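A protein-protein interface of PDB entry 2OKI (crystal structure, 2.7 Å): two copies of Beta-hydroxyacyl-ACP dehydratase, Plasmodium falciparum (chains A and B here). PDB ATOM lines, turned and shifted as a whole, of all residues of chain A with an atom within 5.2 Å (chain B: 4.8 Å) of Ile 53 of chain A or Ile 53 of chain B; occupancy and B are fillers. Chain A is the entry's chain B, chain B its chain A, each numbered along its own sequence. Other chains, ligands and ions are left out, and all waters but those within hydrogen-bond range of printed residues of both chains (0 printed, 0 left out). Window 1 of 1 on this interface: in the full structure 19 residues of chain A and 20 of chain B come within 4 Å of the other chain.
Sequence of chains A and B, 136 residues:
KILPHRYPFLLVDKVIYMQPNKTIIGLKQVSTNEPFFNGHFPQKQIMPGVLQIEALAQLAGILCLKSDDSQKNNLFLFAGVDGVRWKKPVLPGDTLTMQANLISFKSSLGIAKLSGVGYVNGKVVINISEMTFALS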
ATOM      1  N   GLY A  49      14.127 -15.408 -13.123  1.00  0.00           N
ATOM      2  CA  GLY A  49      15.376 -14.702 -13.005  1.00  0.00           C
ATOM      3  C   GLY A  49      15.893 -14.634 -11.593  1.00  0.00           C
ATOM      4  O   GLY A  49      17.101 -14.709 -11.390  1.00  0.00           O
ATOM      5  N   VAL A  50      15.012 -14.504 -10.606  1.00  0.00           N
ATOM      6  CA  VAL A  50      15.493 -14.394  -9.233  1.00  0.00           C
ATOM      7  C   VAL A  50      16.065 -15.675  -8.701  1.00  0.00           C
ATOM      8  O   VAL A  50      16.757 -15.664  -7.684  1.00  0.00           O
ATOM      9  CB  VAL A  50      14.411 -13.906  -8.247  1.00  0.00           C
ATOM     10  CG1 VAL A  50      13.985 -12.496  -8.608  1.00  0.00           C
ATOM     11  CG2 VAL A  50      13.237 -14.862  -8.231  1.00  0.00           C
ATOM     12  N   LEU A  51      15.785 -16.781  -9.383  1.00  0.00           N
ATOM     13  CA  LEU A  51      16.297 -18.080  -8.960  1.00  0.00           C
ATOM     14  C   LEU A  51      17.663 -18.284  -9.541  1.00  0.00           C
ATOM     15  O   LEU A  51      18.416 -19.124  -9.089  1.00  0.00           O
ATOM     16  CB  LEU A  51      15.356 -19.185  -9.394  1.00  0.00           C
ATOM     17  CG  LEU A  51      14.110 -19.179  -8.522  1.00  0.00           C
ATOM     18  CD1 LEU A  51      13.213 -20.310  -8.930  1.00  0.00           C
ATOM     19  CD2 LEU A  51      14.517 -19.306  -7.068  1.00  0.00           C
ATOM     20  N   GLN A  52      17.965 -17.504 -10.566  1.00  0.00           N
ATOM     21  CA  GLN A  52      19.278 -17.536 -11.182  1.00  0.00           C
ATOM     22  C   GLN A  52      20.136 -16.704 -10.219  1.00  0.00           C
ATOM     23  O   GLN A  52      21.280 -17.064  -9.932  1.00  0.00           O
ATOM     24  CB  GLN A  52      19.243 -16.911 -12.583  1.00  0.00           C
ATOM     25  CG  GLN A  52      18.609 -17.805 -13.628  1.00  0.00           C
ATOM     26  CD  GLN A  52      18.138 -17.041 -14.848  1.00  0.00           C
ATOM     27  OE1 GLN A  52      18.918 -16.370 -15.514  1.00  0.00           O
ATOM     28  NE2 GLN A  52      16.850 -17.143 -15.149  1.00  0.00           N
ATOM     29  N   ILE A  53      19.587 -15.605  -9.700  1.00  0.00           N
ATOM     30  CA  ILE A  53      20.346 -14.817  -8.732  1.00  0.00           C
ATOM     31  C   ILE A  53      20.697 -15.729  -7.547  1.00  0.00           C
ATOM     32  O   ILE A  53      21.805 -15.680  -7.022  1.00  0.00           O
ATOM     33  CB  ILE A  53      19.541 -13.604  -8.186  1.00  0.00           C
ATOM     34  CG1 ILE A  53      19.483 -12.495  -9.234  1.00  0.00           C
ATOM     35  CG2 ILE A  53      20.198 -13.058  -6.913  1.00  0.00           C
ATOM     36  CD1 ILE A  53      18.668 -11.283  -8.796  1.00  0.00           C
ATOM     37  N   GLU A  54      19.742 -16.556  -7.135  1.00  0.00           N
ATOM     38  CA  GLU A  54      19.947 -17.470  -6.021  1.00  0.00           C
ATOM     39  C   GLU A  54      20.994 -18.530  -6.361  1.00  0.00           C
ATOM     40  O   GLU A  54      21.780 -18.937  -5.502  1.00  0.00           O
ATOM     41  CB  GLU A  54      18.621 -18.148  -5.653  1.00  0.00           C
ATOM     42  CG  GLU A  54      18.744 -19.211  -4.575  1.00  0.00           C
ATOM     43  CD  GLU A  54      18.990 -18.624  -3.199  1.00  0.00           C
ATOM     44  OE1 GLU A  54      19.565 -19.326  -2.336  1.00  0.00           O
ATOM     45  OE2 GLU A  54      18.592 -17.462  -2.967  1.00  0.00           O
ATOM     46  N   ALA A  55      21.009 -18.960  -7.620  1.00  0.00           N
ATOM     47  CA  ALA A  55      21.927 -19.996  -8.087  1.00  0.00           C
ATOM     48  C   ALA A  55      23.385 -19.571  -8.044  1.00  0.00           C
ATOM     49  O   ALA A  55      24.257 -20.326  -7.591  1.00  0.00           O
ATOM     50  CB  ALA A  55      21.556 -20.414  -9.500  1.00  0.00           C
ATOM     51  N   LEU A  56      23.650 -18.371  -8.543  1.00  0.00           N
ATOM     52  CA  LEU A  56      24.994 -17.850  -8.544  1.00  0.00           C
ATOM     53  C   LEU A  56      25.421 -17.593  -7.113  1.00  0.00           C
ATOM     54  O   LEU A  56      26.551 -17.885  -6.743  1.00  0.00           O
ATOM     55  CB  LEU A  56      25.046 -16.570  -9.363  1.00  0.00           C
ATOM     56  CG  LEU A  56      25.314 -16.812 -10.847  1.00  0.00           C
ATOM     57  CD1 LEU A  56      24.752 -15.680 -11.693  1.00  0.00           C
ATOM     58  CD2 LEU A  56      26.814 -16.965 -11.047  1.00  0.00           C
ATOM     59  N   ALA A  57      24.501 -17.075  -6.302  1.00  0.00           N
ATOM     60  CA  ALA A  57      24.780 -16.759  -4.898  1.00  0.00           C
ATOM     61  C   ALA A  57      25.113 -17.963  -4.010  1.00  0.00           C
ATOM     62  O   ALA A  57      25.733 -17.803  -2.960  1.00  0.00           O
ATOM     63  CB  ALA A  57      23.614 -15.978  -4.304  1.00  0.00           C
ATOM     64  N   PHE A  78      23.880 -14.024   2.636  1.00  0.00           N
ATOM     65  CA  PHE A  78      23.747 -13.256   1.407  1.00  0.00           C
ATOM     66  C   PHE A  78      23.187 -11.940   1.904  1.00  0.00           C
ATOM     67  O   PHE A  78      22.032 -11.874   2.299  1.00  0.00           O
ATOM     68  CB  PHE A  78      22.737 -13.940   0.480  1.00  0.00           C
ATOM     69  CG  PHE A  78      22.778 -13.462  -0.939  1.00  0.00           C
ATOM     70  CD1 PHE A  78      21.670 -13.613  -1.758  1.00  0.00           C
ATOM     71  CD2 PHE A  78      23.919 -12.887  -1.467  1.00  0.00           C
ATOM     72  CE1 PHE A  78      21.696 -13.199  -3.078  1.00  0.00           C
ATOM     73  CE2 PHE A  78      23.952 -12.470  -2.788  1.00  0.00           C
ATOM     74  CZ  PHE A  78      22.835 -12.627  -3.592  1.00  0.00           C
ATOM     75  N   VAL A  81      22.983  -7.358  -3.247  1.00  0.00           N
ATOM     76  CA  VAL A  81      23.373  -7.696  -4.595  1.00  0.00           C
ATOM     77  C   VAL A  81      23.036  -6.558  -5.542  1.00  0.00           C
ATOM     78  O   VAL A  81      22.011  -5.912  -5.389  1.00  0.00           O
ATOM     79  CB  VAL A  81      22.652  -8.980  -5.034  1.00  0.00           C
ATOM     80  CG1 VAL A  81      21.184  -8.677  -5.350  1.00  0.00           C
ATOM     81  CG2 VAL A  81      23.374  -9.600  -6.213  1.00  0.00           C
ATOM     82  N   VAL A  84      22.556  -6.718 -11.685  1.00  0.00           N
ATOM     83  CA  VAL A  84      22.005  -7.942 -12.265  1.00  0.00           C
ATOM     84  C   VAL A  84      21.217  -7.616 -13.523  1.00  0.00           C
ATOM     85  O   VAL A  84      20.396  -6.693 -13.543  1.00  0.00           O
ATOM     86  CB  VAL A  84      21.093  -8.745 -11.266  1.00  0.00           C
ATOM     87  CG1 VAL A  84      21.356  -8.302  -9.837  1.00  0.00           C
ATOM     88  CG2 VAL A  84      19.630  -8.601 -11.635  1.00  0.00           C
ATOM     89  N   TRP A  86      19.315  -9.855 -16.769  1.00  0.00           N
ATOM     90  CA  TRP A  86      18.911 -11.134 -17.346  1.00  0.00           C
ATOM     91  C   TRP A  86      18.735 -10.947 -18.833  1.00  0.00           C
ATOM     92  O   TRP A  86      17.725 -10.399 -19.291  1.00  0.00           O
ATOM     93  CB  TRP A  86      17.591 -11.604 -16.758  1.00  0.00           C
ATOM     94  CG  TRP A  86      17.658 -11.807 -15.309  1.00  0.00           C
ATOM     95  CD1 TRP A  86      18.390 -12.747 -14.646  1.00  0.00           C
ATOM     96  CD2 TRP A  86      17.009 -11.024 -14.312  1.00  0.00           C
ATOM     97  NE1 TRP A  86      18.240 -12.596 -13.292  1.00  0.00           N
ATOM     98  CE2 TRP A  86      17.395 -11.541 -13.058  1.00  0.00           C
ATOM     99  CE3 TRP A  86      16.133  -9.929 -14.353  1.00  0.00           C
ATOM    100  CZ2 TRP A  86      16.942 -11.003 -11.856  1.00  0.00           C
ATOM    101  CZ3 TRP A  86      15.681  -9.394 -13.159  1.00  0.00           C
ATOM    102  CH2 TRP A  86      16.086  -9.933 -11.924  1.00  0.00           C
ATOM    103  N   ILE A 126      22.719 -14.203 -17.882  1.00  0.00           N
ATOM    104  CA  ILE A 126      22.583 -13.346 -16.708  1.00  0.00           C
ATOM    105  C   ILE A 126      23.919 -12.859 -16.159  1.00  0.00           C
ATOM    106  O   ILE A 126      24.833 -13.659 -15.934  1.00  0.00           O
ATOM    107  CB  ILE A 126      21.857 -14.091 -15.565  1.00  0.00           C
ATOM    108  CG1 ILE A 126      21.663 -13.158 -14.368  1.00  0.00           C
ATOM    109  CG2 ILE A 126      22.667 -15.331 -15.150  1.00  0.00           C
ATOM    110  CD1 ILE A 126      21.165 -13.865 -13.118  1.00  0.00           C
ATOM    111  N   ILE A 128      25.997 -10.446 -13.154  1.00  0.00           N
ATOM    112  CA  ILE A 128      25.922  -9.925 -11.791  1.00  0.00           C
ATOM    113  C   ILE A 128      27.245  -9.223 -11.474  1.00  0.00           C
ATOM    114  O   ILE A 128      28.291  -9.862 -11.403  1.00  0.00           O
ATOM    115  CB  ILE A 128      25.703 -11.045 -10.749  1.00  0.00           C
ATOM    116  CG1 ILE A 128      24.527 -11.934 -11.149  1.00  0.00           C
ATOM    117  CG2 ILE A 128      25.406 -10.428  -9.399  1.00  0.00           C
ATOM    118  CD1 ILE A 128      24.130 -12.931 -10.084  1.00  0.00           C
ATOM    119  N   MET A 131      27.994  -9.338  -5.536  1.00  0.00           N
ATOM    120  CA  MET A 131      27.131 -10.035  -4.595  1.00  0.00           C
ATOM    121  C   MET A 131      27.824  -9.935  -3.247  1.00  0.00           C
ATOM    122  O   MET A 131      28.955 -10.388  -3.100  1.00  0.00           O
ATOM    123  CB  MET A 131      26.995 -11.510  -4.964  1.00  0.00           C
ATOM    124  CG  MET A 131      26.445 -11.772  -6.339  1.00  0.00           C
ATOM    125  SD  MET A 131      26.243 -13.535  -6.567  1.00  0.00           S
ATOM    126  CE  MET A 131      27.545 -13.931  -7.754  1.00  0.00           C
ATOM    127  N   GLY B  49      15.467 -13.836   0.755  1.00  0.00           N
ATOM    128  CA  GLY B  49      15.649 -12.472   0.312  1.00  0.00           C
ATOM    129  C   GLY B  49      15.328 -12.310  -1.158  1.00  0.00           C
ATOM    130  O   GLY B  49      14.835 -11.264  -1.590  1.00  0.00           O
ATOM    131  N   VAL B  50      15.602 -13.358  -1.926  1.00  0.00           N
ATOM    132  CA  VAL B  50      15.359 -13.351  -3.359  1.00  0.00           C
ATOM    133  C   VAL B  50      13.877 -13.316  -3.741  1.00  0.00           C
ATOM    134  O   VAL B  50      13.500 -12.631  -4.700  1.00  0.00           O
ATOM    135  CB  VAL B  50      16.057 -14.556  -4.025  1.00  0.00           C
ATOM    136  CG1 VAL B  50      15.369 -14.927  -5.309  1.00  0.00           C
ATOM    137  CG2 VAL B  50      17.506 -14.203  -4.313  1.00  0.00           C
ATOM    138  N   LEU B  51      13.035 -14.037  -3.004  1.00  0.00           N
ATOM    139  CA  LEU B  51      11.605 -14.037  -3.303  1.00  0.00           C
ATOM    140  C   LEU B  51      10.983 -12.733  -2.843  1.00  0.00           C
ATOM    141  O   LEU B  51       9.808 -12.459  -3.086  1.00  0.00           O
ATOM    142  CB  LEU B  51      10.911 -15.221  -2.646  1.00  0.00           C
ATOM    143  CG  LEU B  51      11.367 -16.560  -3.221  1.00  0.00           C
ATOM    144  CD1 LEU B  51      10.475 -17.630  -2.692  1.00  0.00           C
ATOM    145  CD2 LEU B  51      11.311 -16.544  -4.735  1.00  0.00           C
ATOM    146  N   GLN B  52      11.796 -11.924  -2.176  1.00  0.00           N
ATOM    147  CA  GLN B  52      11.371 -10.611  -1.721  1.00  0.00           C
ATOM    148  C   GLN B  52      11.543  -9.615  -2.881  1.00  0.00           C
ATOM    149  O   GLN B  52      10.702  -8.741  -3.081  1.00  0.00           O
ATOM    150  CB  GLN B  52      12.185 -10.186  -0.491  1.00  0.00           C
ATOM    151  CG  GLN B  52      11.599 -10.705   0.821  1.00  0.00           C
ATOM    152  CD  GLN B  52      12.440 -10.386   2.043  1.00  0.00           C
ATOM    153  OE1 GLN B  52      12.899  -9.260   2.231  1.00  0.00           O
ATOM    154  NE2 GLN B  52      12.626 -11.380   2.895  1.00  0.00           N
ATOM    155  N   ILE B  53      12.611  -9.744  -3.667  1.00  0.00           N
ATOM    156  CA  ILE B  53      12.743  -8.805  -4.778  1.00  0.00           C
ATOM    157  C   ILE B  53      11.715  -9.174  -5.857  1.00  0.00           C
ATOM    158  O   ILE B  53      11.316  -8.310  -6.635  1.00  0.00           O
ATOM    159  CB  ILE B  53      14.269  -8.669  -5.372  1.00  0.00           C
ATOM    160  CG1 ILE B  53      14.580  -9.724  -6.419  1.00  0.00           C
ATOM    161  CG2 ILE B  53      15.307  -8.800  -4.250  1.00  0.00           C
ATOM    162  CD1 ILE B  53      16.080  -9.903  -6.656  1.00  0.00           C
ATOM    163  N   GLU B  54      11.265 -10.431  -5.874  1.00  0.00           N
ATOM    164  CA  GLU B  54      10.238 -10.881  -6.828  1.00  0.00           C
ATOM    165  C   GLU B  54       8.896 -10.235  -6.457  1.00  0.00           C
ATOM    166  O   GLU B  54       8.258  -9.577  -7.275  1.00  0.00           O
ATOM    167  CB  GLU B  54      10.083 -12.409  -6.781  1.00  0.00           C
ATOM    168  CG  GLU B  54       8.914 -12.948  -7.603  1.00  0.00           C
ATOM    169  CD  GLU B  54       9.148 -12.850  -9.096  1.00  0.00           C
ATOM    170  OE1 GLU B  54       8.153 -12.787  -9.853  1.00  0.00           O
ATOM    171  OE2 GLU B  54      10.326 -12.855  -9.511  1.00  0.00           O
ATOM    172  N   ALA B  55       8.475 -10.439  -5.213  1.00  0.00           N
ATOM    173  CA  ALA B  55       7.229  -9.871  -4.704  1.00  0.00           C
ATOM    174  C   ALA B  55       7.173  -8.392  -5.040  1.00  0.00           C
ATOM    175  O   ALA B  55       6.144  -7.871  -5.479  1.00  0.00           O
ATOM    176  CB  ALA B  55       7.163 -10.045  -3.191  1.00  0.00           C
ATOM    177  N   LEU B  56       8.304  -7.728  -4.811  1.00  0.00           N
ATOM    178  CA  LEU B  56       8.453  -6.305  -5.059  1.00  0.00           C
ATOM    179  C   LEU B  56       8.526  -6.004  -6.540  1.00  0.00           C
ATOM    180  O   LEU B  56       8.161  -4.914  -6.968  1.00  0.00           O
ATOM    181  CB  LEU B  56       9.715  -5.780  -4.369  1.00  0.00           C
ATOM    182  CG  LEU B  56       9.579  -5.046  -3.030  1.00  0.00           C
ATOM    183  CD1 LEU B  56      10.946  -4.644  -2.539  1.00  0.00           C
ATOM    184  CD2 LEU B  56       8.728  -3.828  -3.199  1.00  0.00           C
ATOM    185  N   ALA B  57       9.008  -6.963  -7.324  1.00  0.00           N
ATOM    186  CA  ALA B  57       9.115  -6.781  -8.769  1.00  0.00           C
ATOM    187  C   ALA B  57       7.746  -6.972  -9.371  1.00  0.00           C
ATOM    188  O   ALA B  57       7.397  -6.335 -10.357  1.00  0.00           O
ATOM    189  CB  ALA B  57      10.085  -7.785  -9.367  1.00  0.00           C
ATOM    190  N   PHE B  78      10.791  -8.073 -16.597  1.00  0.00           N
ATOM    191  CA  PHE B  78      11.754  -7.779 -15.537  1.00  0.00           C
ATOM    192  C   PHE B  78      13.171  -8.055 -16.048  1.00  0.00           C
ATOM    193  O   PHE B  78      13.638  -9.187 -16.033  1.00  0.00           O
ATOM    194  CB  PHE B  78      11.407  -8.641 -14.320  1.00  0.00           C
ATOM    195  CG  PHE B  78      12.120  -8.252 -13.065  1.00  0.00           C
ATOM    196  CD1 PHE B  78      12.430  -6.926 -12.802  1.00  0.00           C
ATOM    197  CD2 PHE B  78      12.477  -9.218 -12.141  1.00  0.00           C
ATOM    198  CE1 PHE B  78      13.091  -6.573 -11.631  1.00  0.00           C
ATOM    199  CE2 PHE B  78      13.136  -8.874 -10.971  1.00  0.00           C
ATOM    200  CZ  PHE B  78      13.446  -7.551 -10.715  1.00  0.00           C
ATOM    201  N   VAL B  81      18.319  -5.728 -11.989  1.00  0.00           N
ATOM    202  CA  VAL B  81      18.154  -5.044 -10.705  1.00  0.00           C
ATOM    203  C   VAL B  81      19.451  -4.565 -10.058  1.00  0.00           C
ATOM    204  O   VAL B  81      20.484  -5.242 -10.118  1.00  0.00           O
ATOM    205  CB  VAL B  81      17.403  -5.930  -9.677  1.00  0.00           C
ATOM    206  CG1 VAL B  81      18.263  -7.112  -9.276  1.00  0.00           C
ATOM    207  CG2 VAL B  81      17.032  -5.112  -8.457  1.00  0.00           C
ATOM    208  N   VAL B  84      20.255  -3.940  -4.053  1.00  0.00           N
ATOM    209  CA  VAL B  84      19.266  -4.612  -3.254  1.00  0.00           C
ATOM    210  C   VAL B  84      19.971  -4.901  -1.947  1.00  0.00           C
ATOM    211  O   VAL B  84      21.015  -5.541  -1.938  1.00  0.00           O
ATOM    212  CB  VAL B  84      18.818  -5.925  -3.912  1.00  0.00           C
ATOM    213  CG1 VAL B  84      17.790  -6.603  -3.037  1.00  0.00           C
ATOM    214  CG2 VAL B  84      18.264  -5.653  -5.305  1.00  0.00           C
ATOM    215  N   TRP B  86      19.337  -6.475   1.877  1.00  0.00           N
ATOM    216  CA  TRP B  86      18.412  -7.207   2.725  1.00  0.00           C
ATOM    217  C   TRP B  86      18.767  -6.845   4.152  1.00  0.00           C
ATOM    218  O   TRP B  86      19.835  -7.206   4.643  1.00  0.00           O
ATOM    219  CB  TRP B  86      18.560  -8.720   2.519  1.00  0.00           C
ATOM    220  CG  TRP B  86      17.960  -9.219   1.238  1.00  0.00           C
ATOM    221  CD1 TRP B  86      16.633  -9.279   0.918  1.00  0.00           C
ATOM    222  CD2 TRP B  86      18.672  -9.679   0.085  1.00  0.00           C
ATOM    223  NE1 TRP B  86      16.477  -9.740  -0.362  1.00  0.00           N
ATOM    224  CE2 TRP B  86      17.711  -9.994  -0.898  1.00  0.00           C
ATOM    225  CE3 TRP B  86      20.032  -9.851  -0.213  1.00  0.00           C
ATOM    226  CZ2 TRP B  86      18.070 -10.476  -2.165  1.00  0.00           C
ATOM    227  CZ3 TRP B  86      20.388 -10.330  -1.469  1.00  0.00           C
ATOM    228  CH2 TRP B  86      19.409 -10.635  -2.429  1.00  0.00           C
ATOM    229  N   ILE B 126      14.177  -4.699   3.577  1.00  0.00           N
ATOM    230  CA  ILE B 126      14.756  -4.882   2.255  1.00  0.00           C
ATOM    231  C   ILE B 126      14.628  -3.634   1.380  1.00  0.00           C
ATOM    232  O   ILE B 126      13.577  -2.982   1.338  1.00  0.00           O
ATOM    233  CB  ILE B 126      14.122  -6.132   1.540  1.00  0.00           C
ATOM    234  CG1 ILE B 126      14.688  -6.282   0.136  1.00  0.00           C
ATOM    235  CG2 ILE B 126      12.610  -6.019   1.487  1.00  0.00           C
ATOM    236  CD1 ILE B 126      14.117  -7.451  -0.612  1.00  0.00           C
ATOM    237  N   ILE B 128      15.685  -1.862  -2.590  1.00  0.00           N
ATOM    238  CA  ILE B 128      16.073  -2.069  -3.977  1.00  0.00           C
ATOM    239  C   ILE B 128      16.112  -0.685  -4.604  1.00  0.00           C
ATOM    240  O   ILE B 128      15.071  -0.042  -4.788  1.00  0.00           O
ATOM    241  CB  ILE B 128      15.072  -2.973  -4.750  1.00  0.00           C
ATOM    242  CG1 ILE B 128      15.037  -4.374  -4.122  1.00  0.00           C
ATOM    243  CG2 ILE B 128      15.491  -3.067  -6.223  1.00  0.00           C
ATOM    244  CD1 ILE B 128      13.946  -5.272  -4.653  1.00  0.00           C
ATOM    245  N   MET B 131      14.900  -1.385 -10.140  1.00  0.00           N
ATOM    246  CA  MET B 131      14.411  -2.566 -10.854  1.00  0.00           C
ATOM    247  C   MET B 131      14.234  -2.094 -12.298  1.00  0.00           C
ATOM    248  O   MET B 131      13.643  -1.042 -12.539  1.00  0.00           O
ATOM    249  CB  MET B 131      13.050  -3.027 -10.310  1.00  0.00           C
ATOM    250  CG  MET B 131      13.040  -3.497  -8.865  1.00  0.00           C
ATOM    251  SD  MET B 131      11.369  -3.869  -8.316  1.00  0.00           S
ATOM    252  CE  MET B 131      10.844  -2.293  -7.663  1.00  0.00           C
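Val 50 of chain A touches Glu 54 of chain B, and with the chains exchanged Glu 54 of chain A touches Val 50 of chain B. Ile 53 of chain A touches its own counterpart, Ile 53 of chain B. Phe 78 of chain A touches Trp 86 of chain B, and with the chains exchanged Trp 86 of chain A touches Phe 78 of chain B. Val 81 of chain A touches Val 84 of chain B, and with the chains exchanged Val 84 of chain A touches Val 81 of chain B. 16 positions are printed for both chains. Of the 11 pairs that touch across the chains among the printed residues, 10 have their exchanged pair printed and touching as well.
CG1 of Val 50 of chain B touches O of Val 50 of chain A, at 2.8 Å. Val 50 of chain A touches Ile 53 of chain B (CG1 to CG1, 3.6 Å). Val 50 of chain A touches Glu 54 of chain B. Ile 53 of chain A touches Val 50 of chain B. CD1 of Ile 53 of chain B touches CD1 of Ile 53 of chain A (3.6 Å). Glu 54 of chain A touches Val 50 of chain B (OE2 to CG2, 3.7 Å). Trp 86 of chain B touches Phe 78 of chain A. CG1 of Val 81 of chain A touches CH2 of Trp 86 of chain B (3.9 Å). CE3 of Trp 86 of chain A touches O of Phe 78 of chain B (3.1 Å).
O of Gly 49 of chain B lies within hydrogen-bond range of NE1 of Trp 86 of chain B. The backbone carbonyl oxygen (O) of Gly 49 of chain A lies within hydrogen-bond range of the indole nitrogen (NE1) of Trp 86 of chain A, at 3.1 Å.
Of the 16 printed residues of chain A, 7 touch a printed residue of chain B. Hydrophobic or aromatic side chains of chain A within 4 Å of the printed part of chain B: Val 50, Ile 53, Phe 78, Val 81, Val 84 and Trp 86. Of the 16 printed residues of chain B, 7 touch a printed residue of chain A. Hydrophobic or aromatic side chains of chain B that line the printed part of chain A: Val 50, Ile 53, Phe 78, Val 81, Val 84 and Trp 86. Among the printed residues, no Asp or Glu carboxylate lies within 4 Å of a Lys or Arg side-chain nitrogen of the other chain.
N of Val 81 of chain B sits at hydrogen-bond distance from O of Val 84 of chain A (2.8 Å). The backbone NH of Val 84 of chain B is in hydrogen-bond range of the backbone carbonyl oxygen of Val 81 of chain A, 3.0 Å away.
Gly 49 of chain A touches none of the printed residues of chain B. Printed residues of chain B within 4 Å of Val 81 of chain A: Val 84 (3.0 Å) and Trp 86 (3.9 Å). Printed residues of chain B within 4 Å of Val 84 of chain A: Val 81. Of the printed residues of chain A, Val 50 of chain B touches Val 50 (2.8 Å), Ile 53 (3.9 Å) and Glu 54 (3.7 Å). Of chain A, only Val 50 and Ile 53 come within 4 Å of Ile 53 of chain B. The nearest residue of chain B that does not touch Ile 53 of chain A is Val 81 of chain B (4.2 Å). The nearest printed residue of chain A that does not touch Val 81 of chain B is Ile 53 of chain A (4.2 Å).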
